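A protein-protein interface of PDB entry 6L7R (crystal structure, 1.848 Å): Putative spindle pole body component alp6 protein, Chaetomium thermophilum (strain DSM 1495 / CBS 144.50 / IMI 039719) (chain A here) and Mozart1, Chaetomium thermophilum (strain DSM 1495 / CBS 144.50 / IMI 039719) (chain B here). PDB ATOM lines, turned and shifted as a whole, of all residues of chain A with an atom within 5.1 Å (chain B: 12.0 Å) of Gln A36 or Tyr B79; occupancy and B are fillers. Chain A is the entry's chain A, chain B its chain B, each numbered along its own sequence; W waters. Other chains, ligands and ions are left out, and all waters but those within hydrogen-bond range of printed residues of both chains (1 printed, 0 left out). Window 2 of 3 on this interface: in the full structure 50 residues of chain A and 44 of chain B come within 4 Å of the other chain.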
ATOM      1  N   ARG A  32      20.250 -12.355  21.687  1.00  0.00           N
ATOM      2  CA  ARG A  32      20.930 -11.750  20.546  1.00  0.00           C
ATOM      3  C   ARG A  32      20.037 -11.730  19.313  1.00  0.00           C
ATOM      4  O   ARG A  32      20.139 -10.813  18.489  1.00  0.00           O
ATOM      5  CB  ARG A  32      22.238 -12.487  20.264  1.00  0.00           C
ATOM      6  CG  ARG A  32      23.197 -12.459  21.450  1.00  0.00           C
ATOM      7  CD  ARG A  32      24.438 -13.293  21.209  1.00  0.00           C
ATOM      8  NE  ARG A  32      25.404 -12.607  20.357  1.00  0.00           N
ATOM      9  CZ  ARG A  32      26.618 -13.075  20.078  1.00  0.00           C
ATOM     10  NH1 ARG A  32      27.018 -14.234  20.583  1.00  0.00           N
ATOM     11  NH2 ARG A  32      27.432 -12.384  19.296  1.00  0.00           N
ATOM     12  N   THR A  33      19.162 -12.726  19.167  1.00  0.00           N
ATOM     13  CA  THR A  33      18.198 -12.690  18.072  1.00  0.00           C
ATOM     14  C   THR A  33      17.184 -11.577  18.286  1.00  0.00           C
ATOM     15  O   THR A  33      16.848 -10.848  17.349  1.00  0.00           O
ATOM     16  CB  THR A  33      17.491 -14.038  17.937  1.00  0.00           C
ATOM     17  OG1 THR A  33      18.454 -15.044  17.628  1.00  0.00           O
ATOM     18  CG2 THR A  33      16.446 -13.992  16.828  1.00  0.00           C
ATOM     19  N   ARG A  34      16.674 -11.446  19.512  1.00  0.00           N
ATOM     20  CA  ARG A  34      15.814 -10.315  19.836  1.00  0.00           C
ATOM     21  C   ARG A  34      16.498  -8.984  19.524  1.00  0.00           C
ATOM     22  O   ARG A  34      15.890  -8.097  18.917  1.00  0.00           O
ATOM     23  CB  ARG A  34      15.422 -10.380  21.309  1.00  0.00           C
ATOM     24  CG  ARG A  34      14.650 -11.642  21.665  1.00  0.00           C
ATOM     25  CD  ARG A  34      14.217 -11.626  23.128  1.00  0.00           C
ATOM     26  NE  ARG A  34      13.502 -12.854  23.464  1.00  0.00           N
ATOM     27  CZ  ARG A  34      13.832 -13.642  24.481  1.00  0.00           C
ATOM     28  NH1 ARG A  34      14.842 -13.325  25.279  1.00  0.00           N
ATOM     29  NH2 ARG A  34      13.134 -14.738  24.722  1.00  0.00           N
ATOM     30  N   ARG A  35      17.771  -8.837  19.907  1.00  0.00           N
ATOM     31  CA  ARG A  35      18.482  -7.592  19.613  1.00  0.00           C
ATOM     32  C   ARG A  35      18.519  -7.308  18.111  1.00  0.00           C
ATOM     33  O   ARG A  35      18.317  -6.165  17.683  1.00  0.00           O
ATOM     34  CB  ARG A  35      19.901  -7.639  20.178  1.00  0.00           C
ATOM     35  CG  ARG A  35      20.773  -6.480  19.683  1.00  0.00           C
ATOM     36  CD  ARG A  35      22.205  -6.518  20.225  1.00  0.00           C
ATOM     37  NE  ARG A  35      22.224  -6.378  21.675  1.00  0.00           N
ATOM     38  CZ  ARG A  35      22.286  -5.211  22.317  1.00  0.00           C
ATOM     39  NH1 ARG A  35      22.330  -4.071  21.634  1.00  0.00           N
ATOM     40  NH2 ARG A  35      22.286  -5.184  23.648  1.00  0.00           N
ATOM     41  N   GLN A  36      18.771  -8.332  17.288  1.00  0.00           N
ATOM     42  CA  GLN A  36      18.811  -8.094  15.849  1.00  0.00           C
ATOM     43  C   GLN A  36      17.443  -7.664  15.325  1.00  0.00           C
ATOM     44  O   GLN A  36      17.347  -6.755  14.488  1.00  0.00           O
ATOM     45  CB  GLN A  36      19.298  -9.346  15.117  1.00  0.00           C
ATOM     46  CG  GLN A  36      19.864  -9.053  13.727  1.00  0.00           C
ATOM     47  CD  GLN A  36      20.955  -7.989  13.749  1.00  0.00           C
ATOM     48  OE1 GLN A  36      21.960  -8.133  14.441  1.00  0.00           O
ATOM     49  NE2 GLN A  36      20.757  -6.914  12.990  1.00  0.00           N
ATOM     50  N   ALA A  37      16.373  -8.306  15.805  1.00  0.00           N
ATOM     51  CA  ALA A  37      15.030  -7.934  15.371  1.00  0.00           C
ATOM     52  C   ALA A  37      14.698  -6.508  15.793  1.00  0.00           C
ATOM     53  O   ALA A  37      14.064  -5.750  15.042  1.00  0.00           O
ATOM     54  CB  ALA A  37      14.006  -8.914  15.953  1.00  0.00           C
ATOM     55  N   VAL A  38      15.109  -6.131  16.999  1.00  0.00           N
ATOM     56  CA  VAL A  38      14.853  -4.773  17.464  1.00  0.00           C
ATOM     57  C   VAL A  38      15.684  -3.789  16.658  1.00  0.00           C
ATOM     58  O   VAL A  38      15.195  -2.730  16.249  1.00  0.00           O
ATOM     59  CB  VAL A  38      15.138  -4.660  18.972  1.00  0.00           C
ATOM     60  CG1 VAL A  38      14.950  -3.230  19.433  1.00  0.00           C
ATOM     61  CG2 VAL A  38      14.213  -5.572  19.750  1.00  0.00           C
ATOM     62  N   PHE A  39      16.943  -4.140  16.393  1.00  0.00           N
ATOM     63  CA  PHE A  39      17.820  -3.259  15.632  1.00  0.00           C
ATOM     64  C   PHE A  39      17.230  -2.969  14.256  1.00  0.00           C
ATOM     65  O   PHE A  39      17.245  -1.823  13.788  1.00  0.00           O
ATOM     66  CB  PHE A  39      19.205  -3.893  15.504  1.00  0.00           C
ATOM     67  CG  PHE A  39      20.215  -3.001  14.849  1.00  0.00           C
ATOM     68  CD1 PHE A  39      20.451  -3.084  13.478  1.00  0.00           C
ATOM     69  CD2 PHE A  39      20.913  -2.067  15.596  1.00  0.00           C
ATOM     70  CE1 PHE A  39      21.386  -2.247  12.858  1.00  0.00           C
ATOM     71  CE2 PHE A  39      21.855  -1.228  14.986  1.00  0.00           C
ATOM     72  CZ  PHE A  39      22.086  -1.322  13.614  1.00  0.00           C
ATOM     73  N   ASP A  40      16.701  -4.005  13.601  1.00  0.00           N
ATOM     74  CA  ASP A  40      16.131  -3.854  12.270  1.00  0.00           C
ATOM     75  C   ASP A  40      14.886  -2.983  12.306  1.00  0.00           C
ATOM     76  O   ASP A  40      14.655  -2.177  11.395  1.00  0.00           O
ATOM     77  CB  ASP A  40      15.806  -5.233  11.685  1.00  0.00           C
ATOM     78  CG  ASP A  40      17.051  -5.996  11.263  1.00  0.00           C
ATOM     79  OD1 ASP A  40      18.170  -5.612  11.683  1.00  0.00           O
ATOM     80  OD2 ASP A  40      16.907  -6.990  10.521  1.00  0.00           O
ATOM     81  N   LEU A  41      14.072  -3.132  13.352  1.00  0.00           N
ATOM     82  CA  LEU A  41      12.919  -2.257  13.527  1.00  0.00           C
ATOM     83  C   LEU A  41      13.353  -0.808  13.706  1.00  0.00           C
ATOM     84  O   LEU A  41      12.788   0.100  13.087  1.00  0.00           O
ATOM     85  CB  LEU A  41      12.092  -2.701  14.727  1.00  0.00           C
ATOM     86  CG  LEU A  41      10.930  -1.762  15.041  1.00  0.00           C
ATOM     87  CD1 LEU A  41       9.882  -1.834  13.945  1.00  0.00           C
ATOM     88  CD2 LEU A  41      10.331  -2.096  16.395  1.00  0.00           C
ATOM     89  N   LEU B  62      10.473   1.026  21.576  1.00  0.00           N
ATOM     90  CA  LEU B  62      11.378   0.325  22.483  1.00  0.00           C
ATOM     91  C   LEU B  62      10.757   0.157  23.863  1.00  0.00           C
ATOM     92  O   LEU B  62      10.924  -0.888  24.506  1.00  0.00           O
ATOM     93  CB  LEU B  62      12.710   1.072  22.602  1.00  0.00           C
ATOM     94  CG  LEU B  62      13.630   1.037  21.374  1.00  0.00           C
ATOM     95  CD1 LEU B  62      14.964   1.690  21.671  1.00  0.00           C
ATOM     96  CD2 LEU B  62      13.838  -0.379  20.935  1.00  0.00           C
ATOM     97  N   LEU B  65       8.285  -2.700  23.575  1.00  0.00           N
ATOM     98  CA  LEU B  65       8.966  -3.988  23.493  1.00  0.00           C
ATOM     99  C   LEU B  65       9.570  -4.383  24.831  1.00  0.00           C
ATOM    100  O   LEU B  65       9.554  -5.562  25.203  1.00  0.00           O
ATOM    101  CB  LEU B  65      10.041  -3.933  22.414  1.00  0.00           C
ATOM    102  CG  LEU B  65       9.458  -3.783  21.013  1.00  0.00           C
ATOM    103  CD1 LEU B  65      10.511  -3.217  20.067  1.00  0.00           C
ATOM    104  CD2 LEU B  65       8.964  -5.154  20.523  1.00  0.00           C
ATOM    105  N   GLN B  70       5.030 -10.364  24.721  1.00  0.00           N
ATOM    106  CA  GLN B  70       4.224 -10.760  23.574  1.00  0.00           C
ATOM    107  C   GLN B  70       4.622  -9.977  22.325  1.00  0.00           C
ATOM    108  O   GLN B  70       4.812 -10.550  21.245  1.00  0.00           O
ATOM    109  CB  GLN B  70       2.747 -10.556  23.912  1.00  0.00           C
ATOM    110  CG  GLN B  70       1.773 -10.706  22.772  1.00  0.00           C
ATOM    111  CD  GLN B  70       0.325 -10.700  23.256  1.00  0.00           C
ATOM    112  OE1 GLN B  70      -0.032  -9.974  24.190  1.00  0.00           O
ATOM    113  NE2 GLN B  70      -0.516 -11.512  22.619  1.00  0.00           N
ATOM    114  N   GLN B  71       4.762  -8.658  22.452  1.00  0.00           N
ATOM    115  CA  GLN B  71       5.122  -7.870  21.279  1.00  0.00           C
ATOM    116  C   GLN B  71       6.573  -8.078  20.874  1.00  0.00           C
ATOM    117  O   GLN B  71       6.882  -8.015  19.680  1.00  0.00           O
ATOM    118  CB  GLN B  71       4.834  -6.385  21.519  1.00  0.00           C
ATOM    119  CG  GLN B  71       3.336  -6.076  21.682  1.00  0.00           C
ATOM    120  CD  GLN B  71       2.495  -6.627  20.555  1.00  0.00           C
ATOM    121  OE1 GLN B  71       2.944  -6.727  19.415  1.00  0.00           O
ATOM    122  NE2 GLN B  71       1.261  -6.986  20.867  1.00  0.00           N
ATOM    123  N   LEU B  72       7.478  -8.328  21.829  1.00  0.00           N
ATOM    124  CA  LEU B  72       8.854  -8.619  21.432  1.00  0.00           C
ATOM    125  C   LEU B  72       8.928  -9.951  20.687  1.00  0.00           C
ATOM    126  O   LEU B  72       9.607 -10.062  19.655  1.00  0.00           O
ATOM    127  CB  LEU B  72       9.784  -8.621  22.646  1.00  0.00           C
ATOM    128  CG  LEU B  72      11.272  -8.883  22.351  1.00  0.00           C
ATOM    129  CD1 LEU B  72      11.836  -7.959  21.253  1.00  0.00           C
ATOM    130  CD2 LEU B  72      12.116  -8.777  23.611  1.00  0.00           C
ATOM    131  N   ASP B  73       8.204 -10.965  21.159  1.00  0.00           N
ATOM    132  CA  ASP B  73       8.256 -12.230  20.432  1.00  0.00           C
ATOM    133  C   ASP B  73       7.556 -12.125  19.084  1.00  0.00           C
ATOM    134  O   ASP B  73       8.002 -12.741  18.108  1.00  0.00           O
ATOM    135  CB  ASP B  73       7.666 -13.366  21.258  1.00  0.00           C
ATOM    136  CG  ASP B  73       8.062 -14.733  20.708  1.00  0.00           C
ATOM    137  OD1 ASP B  73       9.225 -15.154  20.930  1.00  0.00           O
ATOM    138  OD2 ASP B  73       7.216 -15.368  20.041  1.00  0.00           O
ATOM    139  N   ALA B  74       6.493 -11.319  18.991  1.00  0.00           N
ATOM    140  CA  ALA B  74       5.853 -11.127  17.697  1.00  0.00           C
ATOM    141  C   ALA B  74       6.795 -10.423  16.733  1.00  0.00           C
ATOM    142  O   ALA B  74       6.859 -10.773  15.549  1.00  0.00           O
ATOM    143  CB  ALA B  74       4.546 -10.349  17.860  1.00  0.00           C
ATOM    144  N   LEU B  75       7.553  -9.438  17.233  1.00  0.00           N
ATOM    145  CA  LEU B  75       8.562  -8.785  16.406  1.00  0.00           C
ATOM    146  C   LEU B  75       9.595  -9.786  15.887  1.00  0.00           C
ATOM    147  O   LEU B  75       9.970  -9.755  14.704  1.00  0.00           O
ATOM    148  CB  LEU B  75       9.248  -7.681  17.219  1.00  0.00           C
ATOM    149  CG  LEU B  75      10.362  -6.943  16.480  1.00  0.00           C
ATOM    150  CD1 LEU B  75       9.762  -6.146  15.355  1.00  0.00           C
ATOM    151  CD2 LEU B  75      11.174  -6.060  17.406  1.00  0.00           C
ATOM    152  N   VAL B  76      10.075 -10.672  16.761  1.00  0.00           N
ATOM    153  CA  VAL B  76      11.058 -11.676  16.358  1.00  0.00           C
ATOM    154  C   VAL B  76      10.481 -12.594  15.289  1.00  0.00           C
ATOM    155  O   VAL B  76      11.150 -12.910  14.295  1.00  0.00           O
ATOM    156  CB  VAL B  76      11.539 -12.474  17.590  1.00  0.00           C
ATOM    157  CG1 VAL B  76      12.330 -13.699  17.165  1.00  0.00           C
ATOM    158  CG2 VAL B  76      12.379 -11.576  18.521  1.00  0.00           C
ATOM    159  N   ALA B  77       9.233 -13.042  15.478  1.00  0.00           N
ATOM    160  CA  ALA B  77       8.592 -13.898  14.480  1.00  0.00           C
ATOM    161  C   ALA B  77       8.514 -13.204  13.124  1.00  0.00           C
ATOM    162  O   ALA B  77       8.794 -13.814  12.086  1.00  0.00           O
ATOM    163  CB  ALA B  77       7.202 -14.317  14.961  1.00  0.00           C
ATOM    164  N   ASN B  78       8.162 -11.918  13.109  1.00  0.00           N
ATOM    165  CA  ASN B  78       8.123 -11.177  11.850  1.00  0.00           C
ATOM    166  C   ASN B  78       9.511 -11.022  11.247  1.00  0.00           C
ATOM    167  O   ASN B  78       9.679 -11.108  10.022  1.00  0.00           O
ATOM    168  CB  ASN B  78       7.485  -9.806  12.067  1.00  0.00           C
ATOM    169  CG  ASN B  78       6.014  -9.905  12.392  1.00  0.00           C
ATOM    170  OD1 ASN B  78       5.317 -10.776  11.875  1.00  0.00           O
ATOM    171  ND2 ASN B  78       5.533  -9.019  13.255  1.00  0.00           N
ATOM    172  N   TYR B  79      10.519 -10.789  12.090  1.00  0.00           N
ATOM    173  CA  TYR B  79      11.882 -10.637  11.600  1.00  0.00           C
ATOM    174  C   TYR B  79      12.399 -11.939  10.996  1.00  0.00           C
ATOM    175  O   TYR B  79      12.958 -11.944   9.893  1.00  0.00           O
ATOM    176  CB  TYR B  79      12.782 -10.150  12.737  1.00  0.00           C
ATOM    177  CG  TYR B  79      14.253 -10.412  12.534  1.00  0.00           C
ATOM    178  CD1 TYR B  79      15.030  -9.579  11.735  1.00  0.00           C
ATOM    179  CD2 TYR B  79      14.872 -11.487  13.157  1.00  0.00           C
ATOM    180  CE1 TYR B  79      16.385  -9.821  11.555  1.00  0.00           C
ATOM    181  CE2 TYR B  79      16.217 -11.737  12.983  1.00  0.00           C
ATOM    182  CZ  TYR B  79      16.970 -10.904  12.185  1.00  0.00           C
ATOM    183  OH  TYR B  79      18.311 -11.170  12.023  1.00  0.00           O
ATOM    184  N   LEU B  80      12.212 -13.058  11.700  1.00  0.00           N
ATOM    185  CA  LEU B  80      12.695 -14.341  11.192  1.00  0.00           C
ATOM    186  C   LEU B  80      12.011 -14.711   9.881  1.00  0.00           C
ATOM    187  O   LEU B  80      12.638 -15.295   8.989  1.00  0.00           O
ATOM    188  CB  LEU B  80      12.483 -15.436  12.237  1.00  0.00           C
ATOM    189  CG  LEU B  80      13.402 -15.407  13.462  1.00  0.00           C
ATOM    190  CD1 LEU B  80      12.977 -16.449  14.467  1.00  0.00           C
ATOM    191  CD2 LEU B  80      14.854 -15.618  13.058  1.00  0.00           C
ATOM    192  N   ALA B  81      10.730 -14.368   9.736  1.00  0.00           N
ATOM    193  CA  ALA B  81      10.014 -14.671   8.503  1.00  0.00           C
ATOM    194  C   ALA B  81      10.499 -13.835   7.326  1.00  0.00           C
ATOM    195  O   ALA B  81      10.066 -14.081   6.195  1.00  0.00           O
ATOM    196  CB  ALA B  81       8.511 -14.471   8.699  1.00  0.00           C
ATOM    197  N   SER B  82      11.376 -12.863   7.560  1.00  0.00           N
ATOM    198  CA  SER B  82      11.985 -12.093   6.483  1.00  0.00           C
ATOM    199  C   SER B  82      13.451 -12.488   6.327  1.00  0.00           C
ATOM    200  O   SER B  82      13.978 -12.544   5.215  1.00  0.00           O
ATOM    201  CB  SER B  82      11.869 -10.592   6.752  1.00  0.00           C
ATOM    202  OG  SER B  82      10.536 -10.229   7.073  1.00  0.00           O
HETATM  203  O   HOH W   1      11.043 -13.014  22.240  1.00  0.00           O
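No residue of chain B comes within 4 Å of Thr A33.
Arg A35 touches none of the printed residues of chain B.
Gln A36 touches one residue of chain B.
Ala A37 touches two residues of chain B.
Of chain B, only Leu B62, Leu B72 and Leu B75 come within 4 Å of Val A38.
Of chain B, only Tyr B79 comes within 4 Å of Asp A40.
Of the printed residues of chain B, Leu A41 touches Leu B65.
Printed residues of chain A within 4 Å of Leu B62: Val A38.
Of the printed residues of chain A, Leu B72 touches Arg A34 (3.6 Å) and Val A38 (3.7 Å).
Ala B74 touches none of the printed residues of chain A.
Of the printed residues of chain A, Leu B75 touches Ala A37 (3.7 Å) and Val A38 (3.9 Å).
Printed residues of chain A within 4 Å of Val B76: Arg A34 (3.9 Å).
Printed residues of chain A within 4 Å of Tyr B79: Gln A36, Ala A37 and Asp A40.
The nearest printed residue of chain B that does not touch Leu A41 is Leu B75 (4.2 Å).
CD of Arg A34 touches CD2 of Leu B72, at 3.6 Å.
Arg A34 touches Val B76 (CG to CG2, 3.9 Å).
CG of Gln A36 touches OH of Tyr B79, 3.1 Å away.
CD2 of Leu B75 touches O of Ala A37, at 3.7 Å.
CB of Ala A37 touches CB of Tyr B79 (3.7 Å).
Val A38 touches Leu B62.
Leu B72 touches Val A38 (CD1 to CG2, 3.7 Å).
Leu B75 touches Val A38.
Tyr B79 touches Asp A40.
Leu A41 touches Leu B65 (CD2 to CD1, 3.8 Å).
Hydrophobic or aromatic side chains of chain B that line the printed part of chain A: Leu B62, Leu B65, Leu B72, Leu B75, Val B76 and Tyr B79.
Of the 10 printed residues of chain A, 6 touch a printed residue of chain B.
Hydrophobic or aromatic side chains of chain A that line the printed part of chain B: Ala A37, Val A38 and Leu A41.
Among the printed residues, 10 pairs touch across the chains.
Among the printed residues, no Asp or Glu carboxylate lies within 4 Å of a Lys or Arg side-chain nitrogen of the other chain.
Water W1 bridges NE of Arg A34 (2.8 Å) and OD1 of Asp B73 (3.1 Å).
NE2 of Gln A36 sits at hydrogen-bond distance from OD1 of Asp A40 (3.2 Å).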
